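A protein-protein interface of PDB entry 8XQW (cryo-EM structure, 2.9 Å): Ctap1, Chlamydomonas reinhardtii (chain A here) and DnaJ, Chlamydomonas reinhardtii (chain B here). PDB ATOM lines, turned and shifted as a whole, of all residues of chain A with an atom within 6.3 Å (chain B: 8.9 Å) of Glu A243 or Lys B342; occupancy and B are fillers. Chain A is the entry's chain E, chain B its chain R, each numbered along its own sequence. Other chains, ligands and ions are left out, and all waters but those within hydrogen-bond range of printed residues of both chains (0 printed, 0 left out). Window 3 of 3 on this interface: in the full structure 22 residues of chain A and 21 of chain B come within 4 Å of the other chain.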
ATOM      1  N   GLU A 240     -23.834   1.381 -15.193  1.00  0.00           N
ATOM      2  CA  GLU A 240     -24.868   1.203 -16.202  1.00  0.00           C
ATOM      3  C   GLU A 240     -24.352   1.297 -17.628  1.00  0.00           C
ATOM      4  O   GLU A 240     -24.613   2.294 -18.304  1.00  0.00           O
ATOM      5  CB  GLU A 240     -25.967   2.244 -15.975  1.00  0.00           C
ATOM      6  CG  GLU A 240     -27.360   1.848 -16.423  1.00  0.00           C
ATOM      7  CD  GLU A 240     -27.654   2.317 -17.839  1.00  0.00           C
ATOM      8  OE1 GLU A 240     -27.936   1.472 -18.713  1.00  0.00           O
ATOM      9  OE2 GLU A 240     -27.589   3.540 -18.083  1.00  0.00           O
ATOM     10  N   GLU A 241     -23.566   0.322 -18.077  1.00  0.00           N
ATOM     11  CA  GLU A 241     -23.204   0.252 -19.484  1.00  0.00           C
ATOM     12  C   GLU A 241     -24.449   0.439 -20.329  1.00  0.00           C
ATOM     13  O   GLU A 241     -25.342  -0.408 -20.317  1.00  0.00           O
ATOM     14  CB  GLU A 241     -22.565  -1.090 -19.804  1.00  0.00           C
ATOM     15  CG  GLU A 241     -22.367  -1.338 -21.269  1.00  0.00           C
ATOM     16  CD  GLU A 241     -23.242  -2.453 -21.778  1.00  0.00           C
ATOM     17  OE1 GLU A 241     -24.201  -2.822 -21.076  1.00  0.00           O
ATOM     18  OE2 GLU A 241     -22.973  -2.974 -22.876  1.00  0.00           O
ATOM     19  N   GLY A 242     -24.520   1.530 -21.072  1.00  0.00           N
ATOM     20  CA  GLY A 242     -25.806   1.965 -21.571  1.00  0.00           C
ATOM     21  C   GLY A 242     -26.393   1.045 -22.608  1.00  0.00           C
ATOM     22  O   GLY A 242     -27.340   0.312 -22.326  1.00  0.00           O
ATOM     23  N   GLU A 243     -25.832   1.056 -23.801  1.00  0.00           N
ATOM     24  CA  GLU A 243     -26.223   0.131 -24.843  1.00  0.00           C
ATOM     25  C   GLU A 243     -24.973  -0.315 -25.575  1.00  0.00           C
ATOM     26  O   GLU A 243     -24.085   0.486 -25.862  1.00  0.00           O
ATOM     27  CB  GLU A 243     -27.221   0.751 -25.808  1.00  0.00           C
ATOM     28  CG  GLU A 243     -26.711   1.944 -26.553  1.00  0.00           C
ATOM     29  CD  GLU A 243     -27.238   2.000 -27.963  1.00  0.00           C
ATOM     30  OE1 GLU A 243     -26.514   2.483 -28.855  1.00  0.00           O
ATOM     31  OE2 GLU A 243     -28.371   1.535 -28.183  1.00  0.00           O
ATOM     32  N   LEU A 244     -24.897  -1.605 -25.841  1.00  0.00           N
ATOM     33  CA  LEU A 244     -23.687  -2.184 -26.392  1.00  0.00           C
ATOM     34  C   LEU A 244     -23.466  -1.656 -27.800  1.00  0.00           C
ATOM     35  O   LEU A 244     -24.356  -1.750 -28.649  1.00  0.00           O
ATOM     36  CB  LEU A 244     -23.792  -3.703 -26.386  1.00  0.00           C
ATOM     37  CG  LEU A 244     -22.478  -4.468 -26.370  1.00  0.00           C
ATOM     38  CD1 LEU A 244     -21.507  -3.835 -25.412  1.00  0.00           C
ATOM     39  CD2 LEU A 244     -22.732  -5.893 -25.987  1.00  0.00           C
ATOM     40  N   VAL A 245     -22.294  -1.068 -28.038  1.00  0.00           N
ATOM     41  CA  VAL A 245     -21.881  -0.641 -29.364  1.00  0.00           C
ATOM     42  C   VAL A 245     -20.428  -1.033 -29.559  1.00  0.00           C
ATOM     43  O   VAL A 245     -19.676  -1.205 -28.602  1.00  0.00           O
ATOM     44  CB  VAL A 245     -22.042   0.873 -29.589  1.00  0.00           C
ATOM     45  CG1 VAL A 245     -23.439   1.310 -29.283  1.00  0.00           C
ATOM     46  CG2 VAL A 245     -21.063   1.630 -28.748  1.00  0.00           C
ATOM     47  N   GLU A 249     -17.929   3.261 -33.807  1.00  0.00           N
ATOM     48  CA  GLU A 249     -19.338   3.614 -33.909  1.00  0.00           C
ATOM     49  C   GLU A 249     -19.522   5.090 -33.605  1.00  0.00           C
ATOM     50  O   GLU A 249     -19.049   5.578 -32.577  1.00  0.00           O
ATOM     51  CB  GLU A 249     -20.171   2.771 -32.959  1.00  0.00           C
ATOM     52  CG  GLU A 249     -21.528   2.426 -33.491  1.00  0.00           C
ATOM     53  CD  GLU A 249     -22.514   3.545 -33.307  1.00  0.00           C
ATOM     54  OE1 GLU A 249     -23.621   3.476 -33.881  1.00  0.00           O
ATOM     55  OE2 GLU A 249     -22.183   4.502 -32.586  1.00  0.00           O
ATOM     56  N   ALA A 251     -22.810   7.245 -33.523  1.00  0.00           N
ATOM     57  CA  ALA A 251     -24.230   7.551 -33.580  1.00  0.00           C
ATOM     58  C   ALA A 251     -24.785   7.578 -32.168  1.00  0.00           C
ATOM     59  O   ALA A 251     -24.616   6.608 -31.422  1.00  0.00           O
ATOM     60  CB  ALA A 251     -24.983   6.526 -34.427  1.00  0.00           C
ATOM     61  N   PRO A 252     -25.462   8.646 -31.766  1.00  0.00           N
ATOM     62  CA  PRO A 252     -26.010   8.711 -30.417  1.00  0.00           C
ATOM     63  C   PRO A 252     -27.099   7.673 -30.235  1.00  0.00           C
ATOM     64  O   PRO A 252     -27.666   7.176 -31.218  1.00  0.00           O
ATOM     65  CB  PRO A 252     -26.571  10.137 -30.332  1.00  0.00           C
ATOM     66  CG  PRO A 252     -25.925  10.874 -31.447  1.00  0.00           C
ATOM     67  CD  PRO A 252     -25.728   9.874 -32.525  1.00  0.00           C
ATOM     68  N   PRO A 253     -27.497   7.352 -28.976  1.00  0.00           N
ATOM     69  CA  PRO A 253     -28.421   6.252 -28.751  1.00  0.00           C
ATOM     70  C   PRO A 253     -29.918   6.472 -28.703  1.00  0.00           C
ATOM     71  O   PRO A 253     -30.549   5.696 -27.973  1.00  0.00           O
ATOM     72  CB  PRO A 253     -27.894   5.877 -27.365  1.00  0.00           C
ATOM     73  CG  PRO A 253     -27.831   7.183 -26.646  1.00  0.00           C
ATOM     74  CD  PRO A 253     -27.156   8.022 -27.698  1.00  0.00           C
ATOM     75  N   ASP A 258     -29.300   6.698 -22.499  1.00  0.00           N
ATOM     76  CA  ASP A 258     -28.664   5.401 -22.826  1.00  0.00           C
ATOM     77  C   ASP A 258     -27.174   5.610 -23.082  1.00  0.00           C
ATOM     78  O   ASP A 258     -26.619   4.885 -23.910  1.00  0.00           O
ATOM     79  CB  ASP A 258     -29.279   4.803 -24.071  1.00  0.00           C
ATOM     80  CG  ASP A 258     -30.769   5.043 -24.251  1.00  0.00           C
ATOM     81  OD1 ASP A 258     -31.398   5.564 -23.312  1.00  0.00           O
ATOM     82  OD2 ASP A 258     -31.290   4.695 -25.327  1.00  0.00           O
ATOM     83  N   ILE A 259     -26.567   6.591 -22.426  1.00  0.00           N
ATOM     84  CA  ILE A 259     -25.101   6.801 -22.565  1.00  0.00           C
ATOM     85  C   ILE A 259     -24.432   6.158 -21.353  1.00  0.00           C
ATOM     86  O   ILE A 259     -24.627   6.652 -20.242  1.00  0.00           O
ATOM     87  CB  ILE A 259     -24.729   8.280 -22.746  1.00  0.00           C
ATOM     88  CG1 ILE A 259     -25.455   8.887 -23.928  1.00  0.00           C
ATOM     89  CG2 ILE A 259     -23.219   8.448 -22.877  1.00  0.00           C
ATOM     90  CD1 ILE A 259     -24.679   8.784 -25.225  1.00  0.00           C
ATOM     91  N   GLY A 260     -23.722   5.071 -21.572  1.00  0.00           N
ATOM     92  CA  GLY A 260     -23.021   4.341 -20.543  1.00  0.00           C
ATOM     93  C   GLY A 260     -21.543   4.428 -20.793  1.00  0.00           C
ATOM     94  O   GLY A 260     -21.095   5.372 -21.438  1.00  0.00           O
ATOM     95  N   SER A 262     -19.903   2.231 -22.610  1.00  0.00           N
ATOM     96  CA  SER A 262     -19.559   1.709 -23.922  1.00  0.00           C
ATOM     97  C   SER A 262     -19.396   2.837 -24.932  1.00  0.00           C
ATOM     98  O   SER A 262     -18.441   2.841 -25.713  1.00  0.00           O
ATOM     99  CB  SER A 262     -20.611   0.719 -24.385  1.00  0.00           C
ATOM    100  OG  SER A 262     -21.890   1.264 -24.191  1.00  0.00           O
ATOM    101  N   HIS A 263     -20.300   3.815 -24.919  1.00  0.00           N
ATOM    102  CA  HIS A 263     -20.160   4.952 -25.820  1.00  0.00           C
ATOM    103  C   HIS A 263     -18.947   5.794 -25.463  1.00  0.00           C
ATOM    104  O   HIS A 263     -18.231   6.276 -26.348  1.00  0.00           O
ATOM    105  CB  HIS A 263     -21.414   5.808 -25.778  1.00  0.00           C
ATOM    106  CG  HIS A 263     -22.462   5.392 -26.752  1.00  0.00           C
ATOM    107  ND1 HIS A 263     -22.380   5.676 -28.095  1.00  0.00           N
ATOM    108  CD2 HIS A 263     -23.628   4.730 -26.578  1.00  0.00           C
ATOM    109  CE1 HIS A 263     -23.444   5.198 -28.710  1.00  0.00           C
ATOM    110  NE2 HIS A 263     -24.219   4.622 -27.811  1.00  0.00           N
ATOM    111  N   ASP B 335     -36.821  -8.995 -29.862  1.00  0.00           N
ATOM    112  CA  ASP B 335     -36.005  -8.001 -29.175  1.00  0.00           C
ATOM    113  C   ASP B 335     -34.523  -8.301 -29.332  1.00  0.00           C
ATOM    114  O   ASP B 335     -33.722  -7.413 -29.645  1.00  0.00           O
ATOM    115  CB  ASP B 335     -36.376  -7.965 -27.699  1.00  0.00           C
ATOM    116  CG  ASP B 335     -37.715  -7.327 -27.456  1.00  0.00           C
ATOM    117  OD1 ASP B 335     -38.568  -7.395 -28.360  1.00  0.00           O
ATOM    118  OD2 ASP B 335     -37.923  -6.761 -26.363  1.00  0.00           O
ATOM    119  N   THR B 336     -34.139  -9.551 -29.084  1.00  0.00           N
ATOM    120  CA  THR B 336     -32.745  -9.944 -29.218  1.00  0.00           C
ATOM    121  C   THR B 336     -32.268  -9.796 -30.651  1.00  0.00           C
ATOM    122  O   THR B 336     -31.144  -9.345 -30.895  1.00  0.00           O
ATOM    123  CB  THR B 336     -32.569 -11.379 -28.745  1.00  0.00           C
ATOM    124  OG1 THR B 336     -32.946 -11.465 -27.370  1.00  0.00           O
ATOM    125  CG2 THR B 336     -31.139 -11.805 -28.887  1.00  0.00           C
ATOM    126  N   LEU B 337     -33.100 -10.185 -31.616  1.00  0.00           N
ATOM    127  CA  LEU B 337     -32.736  -9.999 -33.014  1.00  0.00           C
ATOM    128  C   LEU B 337     -32.431  -8.539 -33.305  1.00  0.00           C
ATOM    129  O   LEU B 337     -31.429  -8.218 -33.947  1.00  0.00           O
ATOM    130  CB  LEU B 337     -33.856 -10.493 -33.920  1.00  0.00           C
ATOM    131  CG  LEU B 337     -33.789 -11.956 -34.314  1.00  0.00           C
ATOM    132  CD1 LEU B 337     -34.704 -12.220 -35.483  1.00  0.00           C
ATOM    133  CD2 LEU B 337     -32.377 -12.285 -34.668  1.00  0.00           C
ATOM    134  N   ALA B 338     -33.286  -7.636 -32.829  1.00  0.00           N
ATOM    135  CA  ALA B 338     -33.059  -6.219 -33.078  1.00  0.00           C
ATOM    136  C   ALA B 338     -31.770  -5.742 -32.430  1.00  0.00           C
ATOM    137  O   ALA B 338     -30.971  -5.033 -33.057  1.00  0.00           O
ATOM    138  CB  ALA B 338     -34.240  -5.407 -32.569  1.00  0.00           C
ATOM    139  N   ARG B 339     -31.548  -6.127 -31.177  1.00  0.00           N
ATOM    140  CA  ARG B 339     -30.368  -5.660 -30.459  1.00  0.00           C
ATOM    141  C   ARG B 339     -29.090  -6.122 -31.138  1.00  0.00           C
ATOM    142  O   ARG B 339     -28.145  -5.344 -31.309  1.00  0.00           O
ATOM    143  CB  ARG B 339     -30.413  -6.153 -29.021  1.00  0.00           C
ATOM    144  CG  ARG B 339     -29.276  -5.665 -28.180  1.00  0.00           C
ATOM    145  CD  ARG B 339     -29.532  -5.981 -26.732  1.00  0.00           C
ATOM    146  NE  ARG B 339     -29.736  -7.408 -26.546  1.00  0.00           N
ATOM    147  CZ  ARG B 339     -28.771  -8.257 -26.219  1.00  0.00           C
ATOM    148  NH1 ARG B 339     -27.536  -7.815 -26.034  1.00  0.00           N
ATOM    149  NH2 ARG B 339     -29.040  -9.545 -26.070  1.00  0.00           N
ATOM    150  N   LEU B 340     -29.043  -7.387 -31.543  1.00  0.00           N
ATOM    151  CA  LEU B 340     -27.849  -7.887 -32.207  1.00  0.00           C
ATOM    152  C   LEU B 340     -27.660  -7.241 -33.565  1.00  0.00           C
ATOM    153  O   LEU B 340     -26.554  -6.813 -33.898  1.00  0.00           O
ATOM    154  CB  LEU B 340     -27.919  -9.398 -32.351  1.00  0.00           C
ATOM    155  CG  LEU B 340     -27.834 -10.157 -31.041  1.00  0.00           C
ATOM    156  CD1 LEU B 340     -27.603 -11.599 -31.332  1.00  0.00           C
ATOM    157  CD2 LEU B 340     -26.717  -9.596 -30.226  1.00  0.00           C
ATOM    158  N   SER B 341     -28.717  -7.159 -34.370  1.00  0.00           N
ATOM    159  CA  SER B 341     -28.560  -6.565 -35.689  1.00  0.00           C
ATOM    160  C   SER B 341     -28.094  -5.126 -35.600  1.00  0.00           C
ATOM    161  O   SER B 341     -27.412  -4.642 -36.506  1.00  0.00           O
ATOM    162  CB  SER B 341     -29.867  -6.636 -36.461  1.00  0.00           C
ATOM    163  OG  SER B 341     -30.864  -5.893 -35.795  1.00  0.00           O
ATOM    164  N   LYS B 342     -28.446  -4.420 -34.533  1.00  0.00           N
ATOM    165  CA  LYS B 342     -27.917  -3.077 -34.358  1.00  0.00           C
ATOM    166  C   LYS B 342     -26.531  -3.061 -33.744  1.00  0.00           C
ATOM    167  O   LYS B 342     -25.834  -2.051 -33.849  1.00  0.00           O
ATOM    168  CB  LYS B 342     -28.857  -2.240 -33.496  1.00  0.00           C
ATOM    169  CG  LYS B 342     -28.581  -0.752 -33.584  1.00  0.00           C
ATOM    170  CD  LYS B 342     -29.148  -0.003 -32.400  1.00  0.00           C
ATOM    171  CE  LYS B 342     -28.657  -0.578 -31.085  1.00  0.00           C
ATOM    172  NZ  LYS B 342     -27.227  -1.000 -31.127  1.00  0.00           N
ATOM    173  N   TYR B 343     -26.109  -4.144 -33.099  1.00  0.00           N
ATOM    174  CA  TYR B 343     -24.762  -4.179 -32.549  1.00  0.00           C
ATOM    175  C   TYR B 343     -23.719  -4.505 -33.606  1.00  0.00           C
ATOM    176  O   TYR B 343     -22.615  -3.961 -33.558  1.00  0.00           O
ATOM    177  CB  TYR B 343     -24.699  -5.195 -31.418  1.00  0.00           C
ATOM    178  CG  TYR B 343     -23.329  -5.426 -30.860  1.00  0.00           C
ATOM    179  CD1 TYR B 343     -22.650  -4.424 -30.224  1.00  0.00           C
ATOM    180  CD2 TYR B 343     -22.736  -6.658 -30.937  1.00  0.00           C
ATOM    181  CE1 TYR B 343     -21.411  -4.633 -29.704  1.00  0.00           C
ATOM    182  CE2 TYR B 343     -21.495  -6.873 -30.421  1.00  0.00           C
ATOM    183  CZ  TYR B 343     -20.836  -5.856 -29.805  1.00  0.00           C
ATOM    184  OH  TYR B 343     -19.590  -6.067 -29.280  1.00  0.00           O
ATOM    185  N   TRP B 344     -24.044  -5.366 -34.562  1.00  0.00           N
ATOM    186  CA  TRP B 344     -23.105  -5.778 -35.596  1.00  0.00           C
ATOM    187  C   TRP B 344     -23.069  -4.839 -36.785  1.00  0.00           C
ATOM    188  O   TRP B 344     -22.494  -5.198 -37.812  1.00  0.00           O
ATOM    189  CB  TRP B 344     -23.454  -7.171 -36.106  1.00  0.00           C
ATOM    190  CG  TRP B 344     -23.345  -8.233 -35.097  1.00  0.00           C
ATOM    191  CD1 TRP B 344     -22.561  -8.234 -33.999  1.00  0.00           C
ATOM    192  CD2 TRP B 344     -24.039  -9.473 -35.097  1.00  0.00           C
ATOM    193  NE1 TRP B 344     -22.726  -9.396 -33.304  1.00  0.00           N
ATOM    194  CE2 TRP B 344     -23.635 -10.174 -33.961  1.00  0.00           C
ATOM    195  CE3 TRP B 344     -24.976 -10.055 -35.945  1.00  0.00           C
ATOM    196  CZ2 TRP B 344     -24.125 -11.425 -33.653  1.00  0.00           C
ATOM    197  CZ3 TRP B 344     -25.457 -11.293 -35.639  1.00  0.00           C
ATOM    198  CH2 TRP B 344     -25.036 -11.968 -34.501  1.00  0.00           C
ATOM    199  N   ASN B 345     -23.681  -3.668 -36.688  1.00  0.00           N
ATOM    200  CA  ASN B 345     -23.754  -2.719 -37.796  1.00  0.00           C
ATOM    201  C   ASN B 345     -23.430  -1.330 -37.275  1.00  0.00           C
ATOM    202  O   ASN B 345     -24.325  -0.497 -37.098  1.00  0.00           O
ATOM    203  CB  ASN B 345     -25.130  -2.743 -38.454  1.00  0.00           C
ATOM    204  CG  ASN B 345     -25.455  -4.086 -39.042  1.00  0.00           C
ATOM    205  OD1 ASN B 345     -24.737  -4.587 -39.901  1.00  0.00           O
ATOM    206  ND2 ASN B 345     -26.538  -4.686 -38.580  1.00  0.00           N
ATOM    207  N   PRO B 346     -22.162  -1.043 -37.031  1.00  0.00           N
ATOM    208  CA  PRO B 346     -21.795   0.303 -36.601  1.00  0.00           C
ATOM    209  C   PRO B 346     -21.977   1.288 -37.738  1.00  0.00           C
ATOM    210  O   PRO B 346     -21.679   0.997 -38.898  1.00  0.00           O
ATOM    211  CB  PRO B 346     -20.324   0.158 -36.214  1.00  0.00           C
ATOM    212  CG  PRO B 346     -19.840  -0.941 -37.048  1.00  0.00           C
ATOM    213  CD  PRO B 346     -20.980  -1.886 -37.255  1.00  0.00           C
ATOM    214  N   THR B 347     -22.478   2.467 -37.393  1.00  0.00           N
ATOM    215  CA  THR B 347     -22.853   3.477 -38.368  1.00  0.00           C
ATOM    216  C   THR B 347     -21.802   4.574 -38.419  1.00  0.00           C
ATOM    217  O   THR B 347     -21.245   4.963 -37.390  1.00  0.00           O
ATOM    218  CB  THR B 347     -24.217   4.075 -38.023  1.00  0.00           C
ATOM    219  OG1 THR B 347     -25.197   3.032 -37.995  1.00  0.00           O
ATOM    220  CG2 THR B 347     -24.633   5.106 -39.049  1.00  0.00           C
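CE of Lys B342 touches OE2 of Glu A243, at 3.6 Å.
Lys B342 touches Leu A244.
Leu A244 touches Tyr B343 (CG to CE1, 3.5 Å).
CE1 of Tyr B343 touches C of Val A245 (3.7 Å).
CB of Pro B346 touches CG of Glu A249, at 3.7 Å.
Thr B347 touches Glu A249 (N to OE1, 3.8 Å).
Glu A243 touches just one residue of chain B: Lys B342 (3.6 Å).
Lys B342 touches two residues of chain A.
No residue of chain B comes within 4 Å of Gly A242.
Printed residues of chain B within 4 Å of Leu A244: Lys B342 and Tyr B343.
Of the printed residues of chain A, Tyr B343 touches Leu A244 and Val A245.
Printed residues of chain A within 4 Å of Pro B346: Glu A249 (3.7 Å).
Of the printed residues of chain A, Thr B347 touches Glu A249.
Of the printed residues of chain B, Val A245 touches Tyr B343 (3.7 Å).
The nearest residue of chain A that does not touch Lys B342 is Val A245 (4.8 Å).
Of the 13 printed residues of chain B, 4 touch a printed residue of chain A.
Printed residues of chain B that touch a printed residue of chain A: Lys B342, Tyr B343, Pro B346 and Thr B347.
Hydrophobic or aromatic side chains of chain B within 4 Å of the printed part of chain A: Tyr B343 and Pro B346.
Of the 15 printed residues of chain A, 4 touch a printed residue of chain B.
Hydrophobic or aromatic side chains of chain A that line the printed part of chain B: Leu A244.
Among the printed residues, no Asp or Glu carboxylate lies within 4 Å of a Lys or Arg side-chain nitrogen of the other chain.
The side-chain carboxylate (OE1) of Glu A243 sits at hydrogen-bond distance from a ring nitrogen (NE2) of His A263, 3.3 Å away.
The side-chain carboxylate (OE2) of Glu A249 sits at hydrogen-bond distance from the backbone NH (N) of Ala A251 (3.0 Å).
The side-chain hydroxyl (OG) of Ser A262 is in hydrogen-bond range of the backbone carbonyl oxygen (O) of Glu A243, at 2.9 Å.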
